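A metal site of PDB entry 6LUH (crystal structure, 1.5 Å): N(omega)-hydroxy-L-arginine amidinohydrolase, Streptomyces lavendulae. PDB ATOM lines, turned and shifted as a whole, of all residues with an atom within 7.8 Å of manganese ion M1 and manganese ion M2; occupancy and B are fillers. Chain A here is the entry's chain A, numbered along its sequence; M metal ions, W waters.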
ATOM      1  N   THR A  85     -31.049 -26.971  32.461  1.00  0.00           N
ATOM      2  CA  THR A  85     -29.758 -27.343  31.896  1.00  0.00           C
ATOM      3  C   THR A  85     -29.809 -28.757  31.316  1.00  0.00           C
ATOM      4  O   THR A  85     -30.659 -29.580  31.683  1.00  0.00           O
ATOM      5  CB  THR A  85     -28.645 -27.277  32.957  1.00  0.00           C
ATOM      6  OG1 THR A  85     -28.868 -28.281  33.972  1.00  0.00           O
ATOM      7  CG2 THR A  85     -28.575 -25.894  33.615  1.00  0.00           C
ATOM      8  N   CYS A  86     -28.883 -29.033  30.412  1.00  0.00           N
ATOM      9  CA  CYS A  86     -28.733 -30.404  29.933  1.00  0.00           C
ATOM     10  C   CYS A  86     -28.436 -31.375  31.072  1.00  0.00           C
ATOM     11  O   CYS A  86     -28.734 -32.569  30.938  1.00  0.00           O
ATOM     12  CB  CYS A  86     -27.626 -30.493  28.888  1.00  0.00           C
ATOM     13  SG  CYS A  86     -28.001 -29.719  27.327  1.00  0.00           S
ATOM     14  N   SER A  87     -27.820 -30.891  32.155  1.00  0.00           N
ATOM     15  CA  SER A  87     -27.461 -31.792  33.249  1.00  0.00           C
ATOM     16  C   SER A  87     -28.675 -32.452  33.889  1.00  0.00           C
ATOM     17  O   SER A  87     -28.502 -33.520  34.490  1.00  0.00           O
ATOM     18  CB  SER A  87     -26.624 -31.056  34.310  1.00  0.00           C
ATOM     19  OG  SER A  87     -25.443 -30.546  33.722  1.00  0.00           O
ATOM     20  N   TYR A 107     -29.241 -36.424  20.573  1.00  0.00           N
ATOM     21  CA  TYR A 107     -28.713 -35.403  21.485  1.00  0.00           C
ATOM     22  C   TYR A 107     -28.320 -34.207  20.627  1.00  0.00           C
ATOM     23  O   TYR A 107     -27.244 -34.180  20.024  1.00  0.00           O
ATOM     24  CB  TYR A 107     -27.547 -35.964  22.291  1.00  0.00           C
ATOM     25  CG  TYR A 107     -27.227 -35.199  23.552  1.00  0.00           C
ATOM     26  CD1 TYR A 107     -26.513 -34.000  23.499  1.00  0.00           C
ATOM     27  CD2 TYR A 107     -27.604 -35.686  24.792  1.00  0.00           C
ATOM     28  CE1 TYR A 107     -26.215 -33.288  24.662  1.00  0.00           C
ATOM     29  CE2 TYR A 107     -27.308 -34.998  25.956  1.00  0.00           C
ATOM     30  CZ  TYR A 107     -26.591 -33.818  25.882  1.00  0.00           C
ATOM     31  OH  TYR A 107     -26.332 -33.130  27.053  1.00  0.00           O
ATOM     32  N   ILE A 108     -29.226 -33.234  20.542  1.00  0.00           N
ATOM     33  CA  ILE A 108     -29.119 -32.127  19.603  1.00  0.00           C
ATOM     34  C   ILE A 108     -28.508 -30.946  20.347  1.00  0.00           C
ATOM     35  O   ILE A 108     -29.106 -30.396  21.280  1.00  0.00           O
ATOM     36  CB  ILE A 108     -30.483 -31.793  18.980  1.00  0.00           C
ATOM     37  CG1 ILE A 108     -31.138 -33.057  18.408  1.00  0.00           C
ATOM     38  CG2 ILE A 108     -30.295 -30.730  17.900  1.00  0.00           C
ATOM     39  CD1 ILE A 108     -32.528 -32.825  17.815  1.00  0.00           C
ATOM     40  N   ASP A 109     -27.292 -30.564  19.961  1.00  0.00           N
ATOM     41  CA  ASP A 109     -26.476 -29.717  20.818  1.00  0.00           C
ATOM     42  C   ASP A 109     -25.328 -29.198  19.981  1.00  0.00           C
ATOM     43  O   ASP A 109     -24.752 -29.948  19.183  1.00  0.00           O
ATOM     44  CB  ASP A 109     -25.936 -30.529  22.017  1.00  0.00           C
ATOM     45  CG  ASP A 109     -25.496 -29.673  23.196  1.00  0.00           C
ATOM     46  OD1 ASP A 109     -24.814 -28.638  22.989  1.00  0.00           O
ATOM     47  OD2 ASP A 109     -25.739 -30.122  24.343  1.00  0.00           O
ATOM     48  N   GLY A 110     -25.010 -27.915  20.115  1.00  0.00           N
ATOM     49  CA  GLY A 110     -23.800 -27.407  19.485  1.00  0.00           C
ATOM     50  C   GLY A 110     -22.541 -28.010  20.047  1.00  0.00           C
ATOM     51  O   GLY A 110     -21.496 -28.011  19.371  1.00  0.00           O
ATOM     52  N   HIS A 111     -22.616 -28.589  21.256  1.00  0.00           N
ATOM     53  CA  HIS A 111     -21.499 -29.260  21.905  1.00  0.00           C
ATOM     54  C   HIS A 111     -21.687 -30.776  21.890  1.00  0.00           C
ATOM     55  O   HIS A 111     -22.768 -31.301  21.642  1.00  0.00           O
ATOM     56  CB  HIS A 111     -21.371 -28.820  23.361  1.00  0.00           C
ATOM     57  CG  HIS A 111     -21.159 -27.356  23.540  1.00  0.00           C
ATOM     58  ND1 HIS A 111     -22.199 -26.474  23.689  1.00  0.00           N
ATOM     59  CD2 HIS A 111     -20.017 -26.633  23.630  1.00  0.00           C
ATOM     60  CE1 HIS A 111     -21.720 -25.257  23.864  1.00  0.00           C
ATOM     61  NE2 HIS A 111     -20.397 -25.326  23.851  1.00  0.00           N
ATOM     62  N   GLY A 112     -20.585 -31.484  22.211  1.00  0.00           N
ATOM     63  CA  GLY A 112     -20.662 -32.917  22.400  1.00  0.00           C
ATOM     64  C   GLY A 112     -21.120 -33.377  23.776  1.00  0.00           C
ATOM     65  O   GLY A 112     -21.621 -34.498  23.911  1.00  0.00           O
ATOM     66  N   ASP A 113     -20.954 -32.523  24.806  1.00  0.00           N
ATOM     67  CA  ASP A 113     -21.333 -32.849  26.188  1.00  0.00           C
ATOM     68  C   ASP A 113     -20.839 -34.232  26.579  1.00  0.00           C
ATOM     69  O   ASP A 113     -21.523 -34.992  27.281  1.00  0.00           O
ATOM     70  CB  ASP A 113     -22.843 -32.725  26.375  1.00  0.00           C
ATOM     71  CG  ASP A 113     -23.312 -31.272  26.417  1.00  0.00           C
ATOM     72  OD1 ASP A 113     -22.519 -30.335  26.123  1.00  0.00           O
ATOM     73  OD2 ASP A 113     -24.490 -31.091  26.739  1.00  0.00           O
ATOM     74  N   TYR A 124     -17.287 -28.202  34.294  1.00  0.00           N
ATOM     75  CA  TYR A 124     -18.720 -27.930  34.190  1.00  0.00           C
ATOM     76  C   TYR A 124     -19.480 -29.222  33.949  1.00  0.00           C
ATOM     77  O   TYR A 124     -19.229 -29.939  32.967  1.00  0.00           O
ATOM     78  CB  TYR A 124     -18.970 -26.914  33.085  1.00  0.00           C
ATOM     79  CG  TYR A 124     -20.432 -26.614  32.867  1.00  0.00           C
ATOM     80  CD1 TYR A 124     -21.286 -26.379  33.959  1.00  0.00           C
ATOM     81  CD2 TYR A 124     -20.977 -26.572  31.605  1.00  0.00           C
ATOM     82  CE1 TYR A 124     -22.646 -26.104  33.767  1.00  0.00           C
ATOM     83  CE2 TYR A 124     -22.314 -26.313  31.402  1.00  0.00           C
ATOM     84  CZ  TYR A 124     -23.153 -26.088  32.486  1.00  0.00           C
ATOM     85  OH  TYR A 124     -24.500 -25.822  32.256  1.00  0.00           O
ATOM     86  N   GLY A 126     -22.435 -29.656  32.915  1.00  0.00           N
ATOM     87  CA  GLY A 126     -23.187 -29.629  31.677  1.00  0.00           C
ATOM     88  C   GLY A 126     -22.376 -30.080  30.477  1.00  0.00           C
ATOM     89  O   GLY A 126     -22.954 -30.402  29.436  1.00  0.00           O
ATOM     90  N   GLY A 127     -21.045 -30.104  30.596  1.00  0.00           N
ATOM     91  CA  GLY A 127     -20.202 -30.647  29.545  1.00  0.00           C
ATOM     92  C   GLY A 127     -19.982 -32.140  29.629  1.00  0.00           C
ATOM     93  O   GLY A 127     -19.239 -32.686  28.815  1.00  0.00           O
ATOM     94  N   MET A 128     -20.648 -32.812  30.578  1.00  0.00           N
ATOM     95  CA  MET A 128     -20.378 -34.207  30.930  1.00  0.00           C
ATOM     96  C   MET A 128     -21.640 -35.063  30.904  1.00  0.00           C
ATOM     97  O   MET A 128     -21.638 -36.178  31.439  1.00  0.00           O
ATOM     98  CB  MET A 128     -19.752 -34.278  32.333  1.00  0.00           C
ATOM     99  CG  MET A 128     -18.493 -33.405  32.504  1.00  0.00           C
ATOM    100  SD  MET A 128     -18.063 -32.983  34.233  1.00  0.00           S
ATOM    101  CE  MET A 128     -17.649 -34.605  34.870  1.00  0.00           C
ATOM    102  N   VAL A 129     -22.720 -34.570  30.273  1.00  0.00           N
ATOM    103  CA  VAL A 129     -24.022 -35.206  30.417  1.00  0.00           C
ATOM    104  C   VAL A 129     -24.096 -36.499  29.614  1.00  0.00           C
ATOM    105  O   VAL A 129     -24.523 -37.539  30.113  1.00  0.00           O
ATOM    106  CB  VAL A 129     -25.138 -34.232  29.983  1.00  0.00           C
ATOM    107  CG1 VAL A 129     -26.509 -34.907  30.095  1.00  0.00           C
ATOM    108  CG2 VAL A 129     -25.087 -32.941  30.794  1.00  0.00           C
ATOM    109  N   LEU A 130     -23.737 -36.442  28.333  1.00  0.00           N
ATOM    110  CA  LEU A 130     -23.957 -37.611  27.498  1.00  0.00           C
ATOM    111  C   LEU A 130     -22.971 -38.719  27.852  1.00  0.00           C
ATOM    112  O   LEU A 130     -23.336 -39.904  27.853  1.00  0.00           O
ATOM    113  CB  LEU A 130     -23.901 -37.221  26.017  1.00  0.00           C
ATOM    114  CG  LEU A 130     -24.141 -38.332  24.995  1.00  0.00           C
ATOM    115  CD1 LEU A 130     -25.485 -39.009  25.236  1.00  0.00           C
ATOM    116  CD2 LEU A 130     -24.047 -37.788  23.593  1.00  0.00           C
ATOM    117  N   SER A 155     -23.643 -30.867  16.475  1.00  0.00           N
ATOM    118  CA  SER A 155     -22.423 -30.545  17.192  1.00  0.00           C
ATOM    119  C   SER A 155     -21.296 -30.206  16.218  1.00  0.00           C
ATOM    120  O   SER A 155     -21.184 -30.794  15.132  1.00  0.00           O
ATOM    121  CB  SER A 155     -22.005 -31.738  18.068  1.00  0.00           C
ATOM    122  OG  SER A 155     -23.103 -32.399  18.704  1.00  0.00           O
ATOM    123  N   HIS A 196     -33.330 -34.890  22.769  1.00  0.00           N
ATOM    124  CA  HIS A 196     -32.794 -33.960  23.762  1.00  0.00           C
ATOM    125  C   HIS A 196     -32.227 -32.738  23.027  1.00  0.00           C
ATOM    126  O   HIS A 196     -31.353 -32.895  22.172  1.00  0.00           O
ATOM    127  CB  HIS A 196     -31.720 -34.647  24.601  1.00  0.00           C
ATOM    128  CG  HIS A 196     -30.903 -33.733  25.474  1.00  0.00           C
ATOM    129  ND1 HIS A 196     -31.056 -33.684  26.839  1.00  0.00           N
ATOM    130  CD2 HIS A 196     -29.930 -32.832  25.168  1.00  0.00           C
ATOM    131  CE1 HIS A 196     -30.204 -32.805  27.350  1.00  0.00           C
ATOM    132  NE2 HIS A 196     -29.529 -32.257  26.351  1.00  0.00           N
ATOM    133  N   ILE A 197     -32.698 -31.534  23.354  1.00  0.00           N
ATOM    134  CA  ILE A 197     -32.257 -30.347  22.624  1.00  0.00           C
ATOM    135  C   ILE A 197     -31.616 -29.350  23.581  1.00  0.00           C
ATOM    136  O   ILE A 197     -32.252 -28.929  24.557  1.00  0.00           O
ATOM    137  CB  ILE A 197     -33.394 -29.669  21.852  1.00  0.00           C
ATOM    138  CG1 ILE A 197     -33.955 -30.607  20.796  1.00  0.00           C
ATOM    139  CG2 ILE A 197     -32.883 -28.386  21.206  1.00  0.00           C
ATOM    140  CD1 ILE A 197     -35.215 -30.086  20.137  1.00  0.00           C
ATOM    141  N   ASP A 198     -30.378 -28.958  23.275  1.00  0.00           N
ATOM    142  CA  ASP A 198     -29.699 -27.813  23.870  1.00  0.00           C
ATOM    143  C   ASP A 198     -29.755 -26.672  22.851  1.00  0.00           C
ATOM    144  O   ASP A 198     -29.224 -26.800  21.755  1.00  0.00           O
ATOM    145  CB  ASP A 198     -28.276 -28.225  24.228  1.00  0.00           C
ATOM    146  CG  ASP A 198     -27.378 -27.088  24.727  1.00  0.00           C
ATOM    147  OD1 ASP A 198     -27.745 -25.880  24.601  1.00  0.00           O
ATOM    148  OD2 ASP A 198     -26.251 -27.432  25.186  1.00  0.00           O
ATOM    149  N   TRP A 199     -30.404 -25.570  23.216  1.00  0.00           N
ATOM    150  CA  TRP A 199     -30.664 -24.532  22.213  1.00  0.00           C
ATOM    151  C   TRP A 199     -29.417 -23.845  21.677  1.00  0.00           C
ATOM    152  O   TRP A 199     -29.520 -23.149  20.655  1.00  0.00           O
ATOM    153  CB  TRP A 199     -31.618 -23.475  22.777  1.00  0.00           C
ATOM    154  CG  TRP A 199     -33.004 -24.023  23.051  1.00  0.00           C
ATOM    155  CD1 TRP A 199     -33.678 -23.970  24.241  1.00  0.00           C
ATOM    156  CD2 TRP A 199     -33.890 -24.685  22.127  1.00  0.00           C
ATOM    157  NE1 TRP A 199     -34.895 -24.567  24.124  1.00  0.00           N
ATOM    158  CE2 TRP A 199     -35.048 -25.026  22.843  1.00  0.00           C
ATOM    159  CE3 TRP A 199     -33.788 -25.042  20.780  1.00  0.00           C
ATOM    160  CZ2 TRP A 199     -36.132 -25.696  22.251  1.00  0.00           C
ATOM    161  CZ3 TRP A 199     -34.853 -25.717  20.203  1.00  0.00           C
ATOM    162  CH2 TRP A 199     -36.007 -26.044  20.936  1.00  0.00           C
ATOM    163  N   ASP A 200     -28.239 -24.046  22.301  1.00  0.00           N
ATOM    164  CA  ASP A 200     -27.048 -23.474  21.679  1.00  0.00           C
ATOM    165  C   ASP A 200     -26.663 -24.191  20.401  1.00  0.00           C
ATOM    166  O   ASP A 200     -25.706 -23.785  19.743  1.00  0.00           O
ATOM    167  CB  ASP A 200     -25.845 -23.398  22.649  1.00  0.00           C
ATOM    168  CG  ASP A 200     -25.356 -24.763  23.154  1.00  0.00           C
ATOM    169  OD1 ASP A 200     -25.457 -25.757  22.398  1.00  0.00           O
ATOM    170  OD2 ASP A 200     -24.797 -24.811  24.301  1.00  0.00           O
ATOM    171  N   VAL A 201     -27.432 -25.211  20.025  1.00  0.00           N
ATOM    172  CA  VAL A 201     -27.275 -25.810  18.689  1.00  0.00           C
ATOM    173  C   VAL A 201     -27.685 -24.806  17.592  1.00  0.00           C
ATOM    174  O   VAL A 201     -27.216 -24.909  16.448  1.00  0.00           O
ATOM    175  CB  VAL A 201     -28.085 -27.104  18.605  1.00  0.00           C
ATOM    176  CG1 VAL A 201     -29.579 -26.816  18.365  1.00  0.00           C
ATOM    177  CG2 VAL A 201     -27.526 -28.009  17.496  1.00  0.00           C
ATOM    178  N   ALA A 240     -33.914 -27.851  26.562  1.00  0.00           N
ATOM    179  CA  ALA A 240     -32.970 -27.391  27.576  1.00  0.00           C
ATOM    180  C   ALA A 240     -32.181 -26.160  27.126  1.00  0.00           C
ATOM    181  O   ALA A 240     -31.909 -25.968  25.934  1.00  0.00           O
ATOM    182  CB  ALA A 240     -32.004 -28.494  27.961  1.00  0.00           C
ATOM    183  N   GLU A 241     -31.818 -25.352  28.119  1.00  0.00           N
ATOM    184  CA  GLU A 241     -30.846 -24.265  28.000  1.00  0.00           C
ATOM    185  C   GLU A 241     -31.344 -23.111  27.119  1.00  0.00           C
ATOM    186  O   GLU A 241     -30.662 -22.646  26.212  1.00  0.00           O
ATOM    187  CB  GLU A 241     -29.488 -24.802  27.523  1.00  0.00           C
ATOM    188  CG  GLU A 241     -29.051 -25.983  28.419  1.00  0.00           C
ATOM    189  CD  GLU A 241     -27.563 -26.031  28.768  1.00  0.00           C
ATOM    190  OE1 GLU A 241     -26.775 -25.182  28.276  1.00  0.00           O
ATOM    191  OE2 GLU A 241     -27.177 -26.930  29.561  1.00  0.00           O
HETATM  192 MN    MN M   1     -25.741 -29.227  26.347  1.00  0.00          MN
HETATM  193 MN    MN M   2     -24.394 -27.002  24.142  1.00  0.00          MN
HETATM  194  O   HOH W   1     -25.139 -28.311  28.279  1.00  0.00           O
HETATM  195  O   HOH W   2     -23.745 -28.055  25.851  1.00  0.00           O
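The backbone carbonyl oxygen of Asp 109 is in hydrogen-bond range of the side-chain hydroxyl of Ser 155.
The backbone carbonyl oxygen (O) of His 111 sits at hydrogen-bond distance from the side-chain hydroxyl (OG) of Ser 155.
SG of Cys 86 lies close to NE2 of His 196 (3.1 Å).
N of Leu 130 is in hydrogen-bond range of O of Asp 113 (2.8 Å).
OD2 of Asp 113 lies close to OH of Tyr 107 (2.8 Å).
The backbone carbonyl oxygen of Asp 113 sits at hydrogen-bond distance from the backbone NH of Val 129, at 3.3 Å.
OD1 of Asp 200 lies close to N of Gly 110 (3.2 Å).
The backbone NH (N) of Cys 86 lies within hydrogen-bond range of the side-chain carboxylate (OE2) of Glu 241, at 2.8 Å.
Four residues have an atom within 4 Å of manganese ion M1: Cys 86, Asp 109, Asp 113 and Asp 198.
Along chain A the residues within 4 Å of manganese ion M1 span positions 86 to 198.
The nearest printed residue that does not touch manganese ion M1 is Tyr 107 (4.01 Å).
Of the 25 residues printed, 4 come within 4 Å of manganese ion M2.
The nearest printed residue that does not touch manganese ion M2 is Gly 110 (4.2 Å).
Manganese ion M1 is bound by OD2 of Asp 109 (2.2 Å), OD2 of Asp 198 (2.2 Å), water W1 (2.2 Å), OD2 of Asp 113 (2.3 Å), water W2 (2.4 Å) and SG of Cys 86 (2.5 Å).
Manganese ion M2 is bound by OD1 of Asp 109 (2.0 Å).
Water W2 is bound to manganese ion M2, at 2.1 Å.
Manganese ion M2 is bound by the side-chain carboxylate (OD2) of Asp 198 (2.2 Å).
OD2 of Asp 200 is bound to manganese ion M2, at 2.2 Å.
ND1 of His 111 binds manganese ion M2.
The side-chain carboxylate (OD1) of Asp 200 binds manganese ion M2, at 2.4 Å.
Manganese ion M2 has six donor atoms within binding distance.
Water W1 lies within hydrogen-bond range of the side-chain carboxylate of Glu 241 (2.8 Å) and the backbone carbonyl oxygen of Gly 126 (3.2 Å).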
